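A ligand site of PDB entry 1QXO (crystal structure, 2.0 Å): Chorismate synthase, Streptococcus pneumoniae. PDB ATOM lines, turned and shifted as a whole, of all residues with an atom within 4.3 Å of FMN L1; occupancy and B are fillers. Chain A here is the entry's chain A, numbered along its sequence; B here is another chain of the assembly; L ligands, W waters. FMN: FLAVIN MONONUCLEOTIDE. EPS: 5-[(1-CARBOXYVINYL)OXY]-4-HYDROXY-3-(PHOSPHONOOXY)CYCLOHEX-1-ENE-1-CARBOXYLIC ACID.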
ATOM      1  N   ARG A  45      -3.920 -12.974  -1.391  1.00  0.00           N
ATOM      2  CA  ARG A  45      -4.638 -14.067  -2.024  1.00  0.00           C
ATOM      3  C   ARG A  45      -4.869 -13.657  -3.490  1.00  0.00           C
ATOM      4  O   ARG A  45      -5.313 -12.540  -3.735  1.00  0.00           O
ATOM      5  CB  ARG A  45      -5.975 -14.410  -1.384  1.00  0.00           C
ATOM      6  CG  ARG A  45      -5.901 -14.813   0.082  1.00  0.00           C
ATOM      7  CD  ARG A  45      -6.961 -15.838   0.468  1.00  0.00           C
ATOM      8  NE  ARG A  45      -6.633 -17.205   0.102  1.00  0.00           N
ATOM      9  CZ  ARG A  45      -7.438 -18.249   0.230  1.00  0.00           C
ATOM     10  NH1 ARG A  45      -8.674 -18.114   0.709  1.00  0.00           N
ATOM     11  NH2 ARG A  45      -7.063 -19.430  -0.241  1.00  0.00           N
ATOM     12  N   GLY A 109       6.110 -30.179   2.155  1.00  0.00           N
ATOM     13  CA  GLY A 109       5.223 -29.427   2.999  1.00  0.00           C
ATOM     14  C   GLY A 109       3.761 -29.756   2.752  1.00  0.00           C
ATOM     15  O   GLY A 109       2.893 -29.345   3.547  1.00  0.00           O
ATOM     16  N   HIS A 110       3.430 -30.442   1.686  1.00  0.00           N
ATOM     17  CA  HIS A 110       2.034 -30.848   1.448  1.00  0.00           C
ATOM     18  C   HIS A 110       1.754 -32.301   1.786  1.00  0.00           C
ATOM     19  O   HIS A 110       2.662 -33.100   2.073  1.00  0.00           O
ATOM     20  CB  HIS A 110       1.750 -30.605  -0.042  1.00  0.00           C
ATOM     21  CG  HIS A 110       1.135 -29.264  -0.266  1.00  0.00           C
ATOM     22  ND1 HIS A 110      -0.224 -29.045  -0.245  1.00  0.00           N
ATOM     23  CD2 HIS A 110       1.715 -28.063  -0.506  1.00  0.00           C
ATOM     24  CE1 HIS A 110      -0.465 -27.785  -0.483  1.00  0.00           C
ATOM     25  NE2 HIS A 110       0.679 -27.131  -0.594  1.00  0.00           N
ATOM     26  N   ALA A 111       0.481 -32.691   1.620  1.00  0.00           N
ATOM     27  CA  ALA A 111       0.002 -34.021   1.862  1.00  0.00           C
ATOM     28  C   ALA A 111       0.301 -34.995   0.730  1.00  0.00           C
ATOM     29  O   ALA A 111       0.073 -36.215   0.882  1.00  0.00           O
ATOM     30  CB  ALA A 111      -1.542 -34.082   2.037  1.00  0.00           C
ATOM     31  N   SER A 131      -6.956 -32.671   0.079  1.00  0.00           N
ATOM     32  CA  SER A 131      -6.169 -32.017   1.128  1.00  0.00           C
ATOM     33  C   SER A 131      -6.153 -30.506   1.014  1.00  0.00           C
ATOM     34  O   SER A 131      -5.862 -29.778   1.960  1.00  0.00           O
ATOM     35  CB  SER A 131      -4.679 -32.472   1.103  1.00  0.00           C
ATOM     36  OG  SER A 131      -4.011 -31.996  -0.067  1.00  0.00           O
ATOM     37  N   ALA A 133      -6.876 -26.665   0.987  1.00  0.00           N
ATOM     38  CA  ALA A 133      -7.657 -25.791   1.841  1.00  0.00           C
ATOM     39  C   ALA A 133      -8.903 -25.245   1.193  1.00  0.00           C
ATOM     40  O   ALA A 133      -9.683 -24.538   1.856  1.00  0.00           O
ATOM     41  CB  ALA A 133      -6.794 -24.772   2.561  1.00  0.00           C
ATOM     42  N   THR A 136     -11.731 -25.611   3.511  1.00  0.00           N
ATOM     43  CA  THR A 136     -12.043 -24.773   4.643  1.00  0.00           C
ATOM     44  C   THR A 136     -13.278 -23.907   4.377  1.00  0.00           C
ATOM     45  O   THR A 136     -13.876 -23.419   5.335  1.00  0.00           O
ATOM     46  CB  THR A 136     -10.852 -23.906   5.076  1.00  0.00           C
ATOM     47  OG1 THR A 136     -10.448 -23.010   4.019  1.00  0.00           O
ATOM     48  CG2 THR A 136      -9.621 -24.744   5.393  1.00  0.00           C
ATOM     49  N   ILE A 250      -6.652 -27.245  11.356  1.00  0.00           N
ATOM     50  CA  ILE A 250      -6.710 -26.349  10.173  1.00  0.00           C
ATOM     51  C   ILE A 250      -5.419 -26.553   9.385  1.00  0.00           C
ATOM     52  O   ILE A 250      -4.306 -26.683   9.940  1.00  0.00           O
ATOM     53  CB  ILE A 250      -6.935 -24.912  10.590  1.00  0.00           C
ATOM     54  CG1 ILE A 250      -8.174 -24.825  11.524  1.00  0.00           C
ATOM     55  CG2 ILE A 250      -7.167 -23.930   9.414  1.00  0.00           C
ATOM     56  CD1 ILE A 250      -8.280 -23.426  12.139  1.00  0.00           C
ATOM     57  N   ASN A 251      -5.575 -26.674   8.056  1.00  0.00           N
ATOM     58  CA  ASN A 251      -4.430 -26.813   7.161  1.00  0.00           C
ATOM     59  C   ASN A 251      -3.351 -25.801   7.507  1.00  0.00           C
ATOM     60  O   ASN A 251      -3.658 -24.632   7.721  1.00  0.00           O
ATOM     61  CB  ASN A 251      -4.911 -26.429   5.711  1.00  0.00           C
ATOM     62  CG  ASN A 251      -5.838 -27.483   5.158  1.00  0.00           C
ATOM     63  OD1 ASN A 251      -6.823 -27.799   5.842  1.00  0.00           O
ATOM     64  ND2 ASN A 251      -5.652 -28.029   3.967  1.00  0.00           N
ATOM     65  N   ALA A 252      -2.095 -26.236   7.626  1.00  0.00           N
ATOM     66  CA  ALA A 252      -0.939 -25.413   7.830  1.00  0.00           C
ATOM     67  C   ALA A 252      -0.791 -25.020   9.275  1.00  0.00           C
ATOM     68  O   ALA A 252       0.251 -24.432   9.593  1.00  0.00           O
ATOM     69  CB  ALA A 252      -0.819 -24.176   6.925  1.00  0.00           C
ATOM     70  N   PHE A 253      -1.746 -25.333  10.151  1.00  0.00           N
ATOM     71  CA  PHE A 253      -1.537 -24.932  11.553  1.00  0.00           C
ATOM     72  C   PHE A 253      -0.592 -25.888  12.274  1.00  0.00           C
ATOM     73  O   PHE A 253      -0.766 -27.073  12.209  1.00  0.00           O
ATOM     74  CB  PHE A 253      -2.819 -24.757  12.395  1.00  0.00           C
ATOM     75  CG  PHE A 253      -3.493 -23.421  12.128  1.00  0.00           C
ATOM     76  CD1 PHE A 253      -3.862 -23.074  10.836  1.00  0.00           C
ATOM     77  CD2 PHE A 253      -3.738 -22.499  13.142  1.00  0.00           C
ATOM     78  CE1 PHE A 253      -4.512 -21.867  10.567  1.00  0.00           C
ATOM     79  CE2 PHE A 253      -4.389 -21.310  12.896  1.00  0.00           C
ATOM     80  CZ  PHE A 253      -4.787 -20.968  11.562  1.00  0.00           C
ATOM     81  N   MET A 310       0.227 -20.495  11.977  1.00  0.00           N
ATOM     82  CA  MET A 310       0.025 -21.053  10.636  1.00  0.00           C
ATOM     83  C   MET A 310       1.395 -21.070   9.966  1.00  0.00           C
ATOM     84  O   MET A 310       2.029 -20.000  10.034  1.00  0.00           O
ATOM     85  CB  MET A 310      -0.869 -20.172   9.768  1.00  0.00           C
ATOM     86  CG  MET A 310      -1.082 -20.864   8.437  1.00  0.00           C
ATOM     87  SD  MET A 310      -1.800 -19.446   7.098  1.00  0.00           S
ATOM     88  CE  MET A 310      -2.516 -20.613   5.780  1.00  0.00           C
ATOM     89  N   LYS A 311       1.903 -22.213   9.572  1.00  0.00           N
ATOM     90  CA  LYS A 311       3.198 -22.180   8.848  1.00  0.00           C
ATOM     91  C   LYS A 311       2.976 -21.498   7.504  1.00  0.00           C
ATOM     92  O   LYS A 311       1.829 -21.377   7.047  1.00  0.00           O
ATOM     93  CB  LYS A 311       3.678 -23.622   8.674  1.00  0.00           C
ATOM     94  CG  LYS A 311       3.128 -24.324   7.430  1.00  0.00           C
ATOM     95  CD  LYS A 311       3.376 -25.846   7.571  1.00  0.00           C
ATOM     96  CE  LYS A 311       3.147 -26.409   6.133  1.00  0.00           C
ATOM     97  NZ  LYS A 311       2.928 -27.881   6.218  1.00  0.00           N
ATOM     98  N   ILE A 313       2.624 -20.950   3.512  1.00  0.00           N
ATOM     99  CA  ILE A 313       2.123 -21.714   2.398  1.00  0.00           C
ATOM    100  C   ILE A 313       3.352 -22.497   1.920  1.00  0.00           C
ATOM    101  O   ILE A 313       4.338 -21.841   1.608  1.00  0.00           O
ATOM    102  CB  ILE A 313       1.707 -20.775   1.217  1.00  0.00           C
ATOM    103  CG1 ILE A 313       0.437 -20.013   1.468  1.00  0.00           C
ATOM    104  CG2 ILE A 313       1.708 -21.499  -0.142  1.00  0.00           C
ATOM    105  CD1 ILE A 313      -0.639 -20.687   2.304  1.00  0.00           C
ATOM    106  N   PRO A 314       3.205 -23.775   1.687  1.00  0.00           N
ATOM    107  CA  PRO A 314       4.301 -24.614   1.219  1.00  0.00           C
ATOM    108  C   PRO A 314       4.730 -24.387  -0.219  1.00  0.00           C
ATOM    109  O   PRO A 314       5.918 -24.599  -0.522  1.00  0.00           O
ATOM    110  CB  PRO A 314       3.792 -26.035   1.367  1.00  0.00           C
ATOM    111  CG  PRO A 314       2.633 -25.932   2.314  1.00  0.00           C
ATOM    112  CD  PRO A 314       2.026 -24.556   2.083  1.00  0.00           C
ATOM    113  N   THR A 315       3.838 -24.003  -1.120  1.00  0.00           N
ATOM    114  CA  THR A 315       4.264 -23.828  -2.519  1.00  0.00           C
ATOM    115  C   THR A 315       5.049 -22.548  -2.755  1.00  0.00           C
ATOM    116  O   THR A 315       4.536 -21.443  -2.547  1.00  0.00           O
ATOM    117  CB  THR A 315       3.036 -23.830  -3.433  1.00  0.00           C
ATOM    118  OG1 THR A 315       2.254 -22.715  -2.983  1.00  0.00           O
ATOM    119  CG2 THR A 315       2.184 -25.063  -3.329  1.00  0.00           C
ATOM    120  N   ALA A 342      -1.810 -16.653   2.996  1.00  0.00           N
ATOM    121  CA  ALA A 342      -3.254 -16.810   3.148  1.00  0.00           C
ATOM    122  C   ALA A 342      -3.583 -16.681   4.634  1.00  0.00           C
ATOM    123  O   ALA A 342      -4.609 -17.179   5.132  1.00  0.00           O
ATOM    124  CB  ALA A 342      -3.715 -18.122   2.528  1.00  0.00           C
ATOM    125  N   ALA A 345      -7.245 -15.078   5.741  1.00  0.00           N
ATOM    126  CA  ALA A 345      -8.274 -16.097   5.453  1.00  0.00           C
ATOM    127  C   ALA A 345      -8.201 -17.235   6.471  1.00  0.00           C
ATOM    128  O   ALA A 345      -9.218 -17.653   7.030  1.00  0.00           O
ATOM    129  CB  ALA A 345      -8.099 -16.526   4.017  1.00  0.00           C
ATOM    130  N   ALA A 346      -6.993 -17.643   6.858  1.00  0.00           N
ATOM    131  CA  ALA A 346      -6.807 -18.676   7.865  1.00  0.00           C
ATOM    132  C   ALA A 346      -7.375 -18.236   9.224  1.00  0.00           C
ATOM    133  O   ALA A 346      -7.860 -19.036  10.030  1.00  0.00           O
ATOM    134  CB  ALA A 346      -5.312 -18.989   8.054  1.00  0.00           C
ATOM    135  N   GLU B 295       2.683 -34.123   7.842  1.00  0.00           N
ATOM    136  CA  GLU B 295       2.358 -33.467   6.570  1.00  0.00           C
ATOM    137  C   GLU B 295       0.903 -33.823   6.282  1.00  0.00           C
ATOM    138  O   GLU B 295       0.542 -35.007   6.325  1.00  0.00           O
ATOM    139  CB  GLU B 295       3.241 -34.034   5.448  1.00  0.00           C
ATOM    140  CG  GLU B 295       4.678 -33.496   5.548  1.00  0.00           C
ATOM    141  CD  GLU B 295       5.612 -34.355   4.702  1.00  0.00           C
ATOM    142  OE1 GLU B 295       5.219 -35.293   3.946  1.00  0.00           O
ATOM    143  OE2 GLU B 295       6.801 -34.044   4.811  1.00  0.00           O
ATOM    144  N   GLY B 296       0.001 -32.845   6.226  1.00  0.00           N
ATOM    145  CA  GLY B 296      -1.401 -33.066   5.987  1.00  0.00           C
ATOM    146  C   GLY B 296      -2.052 -33.802   7.174  1.00  0.00           C
ATOM    147  O   GLY B 296      -2.992 -34.573   6.941  1.00  0.00           O
ATOM    148  N   GLY B 297      -1.543 -33.676   8.378  1.00  0.00           N
ATOM    149  CA  GLY B 297      -2.190 -34.385   9.507  1.00  0.00           C
ATOM    150  C   GLY B 297      -1.785 -35.861   9.512  1.00  0.00           C
ATOM    151  O   GLY B 297      -2.320 -36.602  10.339  1.00  0.00           O
HETATM  152  N1  FMN L   1      -0.986 -24.110   0.753  1.00  0.00           N
HETATM  153  C2  FMN L   1      -0.465 -23.958  -0.495  1.00  0.00           C
HETATM  154  O2  FMN L   1       0.490 -24.591  -0.854  1.00  0.00           O
HETATM  155  N3  FMN L   1      -1.089 -23.040  -1.344  1.00  0.00           N
HETATM  156  C4  FMN L   1      -2.120 -22.274  -1.114  1.00  0.00           C
HETATM  157  O4  FMN L   1      -2.625 -21.477  -1.904  1.00  0.00           O
HETATM  158  C4A FMN L   1      -2.692 -22.425   0.247  1.00  0.00           C
HETATM  159  N5  FMN L   1      -3.813 -21.887   0.592  1.00  0.00           N
HETATM  160  C5A FMN L   1      -4.288 -22.033   1.887  1.00  0.00           C
HETATM  161  C6  FMN L   1      -5.356 -21.237   2.350  1.00  0.00           C
HETATM  162  C7  FMN L   1      -5.864 -21.356   3.632  1.00  0.00           C
HETATM  163  C7M FMN L   1      -7.050 -20.483   4.137  1.00  0.00           C
HETATM  164  C8  FMN L   1      -5.313 -22.306   4.511  1.00  0.00           C
HETATM  165  C8M FMN L   1      -5.865 -22.436   5.927  1.00  0.00           C
HETATM  166  C9  FMN L   1      -4.252 -23.113   4.073  1.00  0.00           C
HETATM  167  C9A FMN L   1      -3.730 -22.962   2.761  1.00  0.00           C
HETATM  168  N10 FMN L   1      -2.565 -23.582   2.337  1.00  0.00           N
HETATM  169  C10 FMN L   1      -2.028 -23.406   1.112  1.00  0.00           C
HETATM  170  C1' FMN L   1      -1.871 -24.600   3.185  1.00  0.00           C
HETATM  171  C2' FMN L   1      -2.037 -26.040   2.852  1.00  0.00           C
HETATM  172  O2' FMN L   1      -3.460 -26.369   2.720  1.00  0.00           O
HETATM  173  C3' FMN L   1      -1.460 -27.101   3.865  1.00  0.00           C
HETATM  174  O3' FMN L   1      -0.083 -26.818   4.307  1.00  0.00           O
HETATM  175  C4' FMN L   1      -1.369 -28.520   3.364  1.00  0.00           C
HETATM  176  O4' FMN L   1      -2.677 -29.041   3.067  1.00  0.00           O
HETATM  177  C5' FMN L   1      -0.652 -29.540   4.258  1.00  0.00           C
HETATM  178  O5' FMN L   1      -1.273 -29.571   5.611  1.00  0.00           O
HETATM  179  P   FMN L   1      -0.443 -29.082   6.869  1.00  0.00           P
HETATM  180  O1P FMN L   1       0.310 -27.818   6.560  1.00  0.00           O
HETATM  181  O2P FMN L   1       0.544 -30.207   7.170  1.00  0.00           O
HETATM  182  O3P FMN L   1      -1.573 -28.916   7.915  1.00  0.00           O
HETATM  183  C1  EPS L   2      -4.570 -24.427  -2.029  1.00  0.00           C
HETATM  184  C2  EPS L   2      -4.265 -24.214  -3.412  1.00  0.00           C
HETATM  185  C3  EPS L   2      -4.889 -23.249  -4.225  1.00  0.00           C
HETATM  186  C4  EPS L   2      -5.534 -22.359  -3.302  1.00  0.00           C
HETATM  187  C5  EPS L   2      -6.476 -23.058  -2.488  1.00  0.00           C
HETATM  188  C6  EPS L   2      -5.743 -23.780  -1.499  1.00  0.00           C
HETATM  189  O3  EPS L   2      -5.830 -23.863  -4.852  1.00  0.00           O
HETATM  190  P   EPS L   2      -5.284 -23.723  -6.352  1.00  0.00           P
HETATM  191  O1P EPS L   2      -3.777 -24.043  -6.497  1.00  0.00           O
HETATM  192  O2P EPS L   2      -6.432 -24.193  -7.363  1.00  0.00           O
HETATM  193  O3P EPS L   2      -5.428 -22.081  -6.620  1.00  0.00           O
HETATM  194  O4  EPS L   2      -5.975 -21.377  -4.042  1.00  0.00           O
HETATM  195  O5  EPS L   2      -7.322 -22.157  -1.870  1.00  0.00           O
HETATM  196  C7  EPS L   2      -8.644 -22.054  -2.200  1.00  0.00           C
HETATM  197  C8  EPS L   2      -9.127 -22.511  -3.477  1.00  0.00           C
HETATM  198  C9  EPS L   2      -9.615 -21.525  -1.373  1.00  0.00           C
HETATM  199  O91 EPS L   2      -9.315 -21.049  -0.216  1.00  0.00           O
HETATM  200  O92 EPS L   2     -10.896 -21.518  -1.662  1.00  0.00           O
HETATM  201  C10 EPS L   2      -4.063 -25.347  -1.085  1.00  0.00           C
HETATM  202  O11 EPS L   2      -4.391 -25.438   0.194  1.00  0.00           O
HETATM  203  O12 EPS L   2      -3.180 -26.307  -1.217  1.00  0.00           O
HETATM  204  O   HOH W   1      -2.236 -28.848  10.700  1.00  0.00           O
HETATM  205  O   HOH W   2      -3.277 -28.369   0.320  1.00  0.00           O
HETATM  206  O   HOH W   3      -1.657 -20.157  -4.206  1.00  0.00           O
HETATM  207  O   HOH W   4      -3.608 -30.507   7.391  1.00  0.00           O
HETATM  208  O   HOH W   5      -4.259 -19.123  -0.920  1.00  0.00           O
HETATM  209  O   HOH W   6      -0.735 -23.147  -4.325  1.00  0.00           O
HETATM  210  O   HOH W   7       2.985 -29.965   8.248  1.00  0.00           O
HETATM  211  O   HOH W   8       0.281 -31.763   9.639  1.00  0.00           O
HETATM  212  O   HOH W   9      -3.992 -30.981   4.598  1.00  0.00           O
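An oxygen (O2') of FMN L1 sits at hydrogen-bond distance from the side-chain amide nitrogen (ND2) of Asn 251 (3.0 Å). The backbone NH of Ala 252 is in hydrogen-bond range of an oxygen (O3P) of FMN L1 (2.7 Å). An oxygen (O11) of EPS L2 is in hydrogen-bond range of the backbone NH (N) of Ala 133 (2.9 Å). NZ of Lys 311 is in salt-bridge range of O1P of FMN L1 (2.6 Å). OG1 of Thr 315 sits close to O2 of FMN L1, at 3.3 Å. N of Thr 315 sits close to O2 of FMN L1, 3.4 Å away. The backbone carbonyl oxygen (O) of Ser 131 is in hydrogen-bond range of an oxygen (O4') of FMN L1, at 3.5 Å. The backbone NH of Gly 296 of chain B sits at hydrogen-bond distance from an oxygen (O2P) of FMN L1, 2.9 Å away. The guanidinium group (NH2) of Arg 45 is in salt-bridge range of an oxygen (O91) of EPS L2 (2.8 Å). An oxygen (O2) of FMN L1 is in hydrogen-bond range of a ring nitrogen (NE2) of His 110 (2.6 Å).
Water W7 lies within hydrogen-bond range of O2P of FMN L1 (2.7 Å) and NZ of Lys 311 (2.9 Å). Water W9 lies within hydrogen-bond range of O4' of FMN L1 (2.8 Å), ND2 of Asn 251 (3.4 Å) and O of Ser 131 (3.5 Å). Water W1 lies within hydrogen-bond range of the backbone carbonyl oxygen (O) of Phe 253 (2.8 Å), an oxygen (O3P) of FMN L1 (2.9 Å) and the backbone carbonyl oxygen (O) of Ile 250 (3.1 Å). Water W2 lies within hydrogen-bond range of an oxygen (O12) of EPS L2, an oxygen (O4') of FMN L1, a ring nitrogen (ND1) of His 110 and the backbone carbonyl oxygen (O) of Ser 131. Water W8 bridges the backbone NH of Gly 297 of chain B (2.9 Å) and an oxygen (O2P) of FMN L1 (2.9 Å). Water W5 bridges NH2 of Arg 45 and O4 of FMN L1.
Residues that only touch FMN L1: Ile 313, Pro 314, Ala 133, Met 310, Ala 342, Arg 45, Gly 109, Glu 295 of chain B and Ala 346. Hydrophobic or aromatic side chains that line FMN L1: His 110, Ala 133, Ala 252, Met 310, Ile 313, Pro 314 and Ala 342. Of the 22 residues printed, 16 come within 4 Å of FMN L1. The nearest printed residue that does not touch FMN L1 is Ile 250 (4.01 Å).
ND2 of Asn 251 sits at hydrogen-bond distance from O of Ser 131, 2.7 Å away. The backbone carbonyl oxygen of Gly 109 sits at hydrogen-bond distance from the side-chain amino group of Lys 311 (3.0 Å). ND2 of Asn 251 lies close to N of Ala 133. The side-chain hydroxyl of Thr 136 sits at hydrogen-bond distance from the backbone carbonyl oxygen of Ala 133, 2.8 Å away. The backbone NH of Lys 311 lies within hydrogen-bond range of the backbone carbonyl oxygen of Ala 252, 2.8 Å away.
An oxygen (O2') of FMN L1 sits at hydrogen-bond distance from an oxygen (O11) of EPS L2 (2.8 Å).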
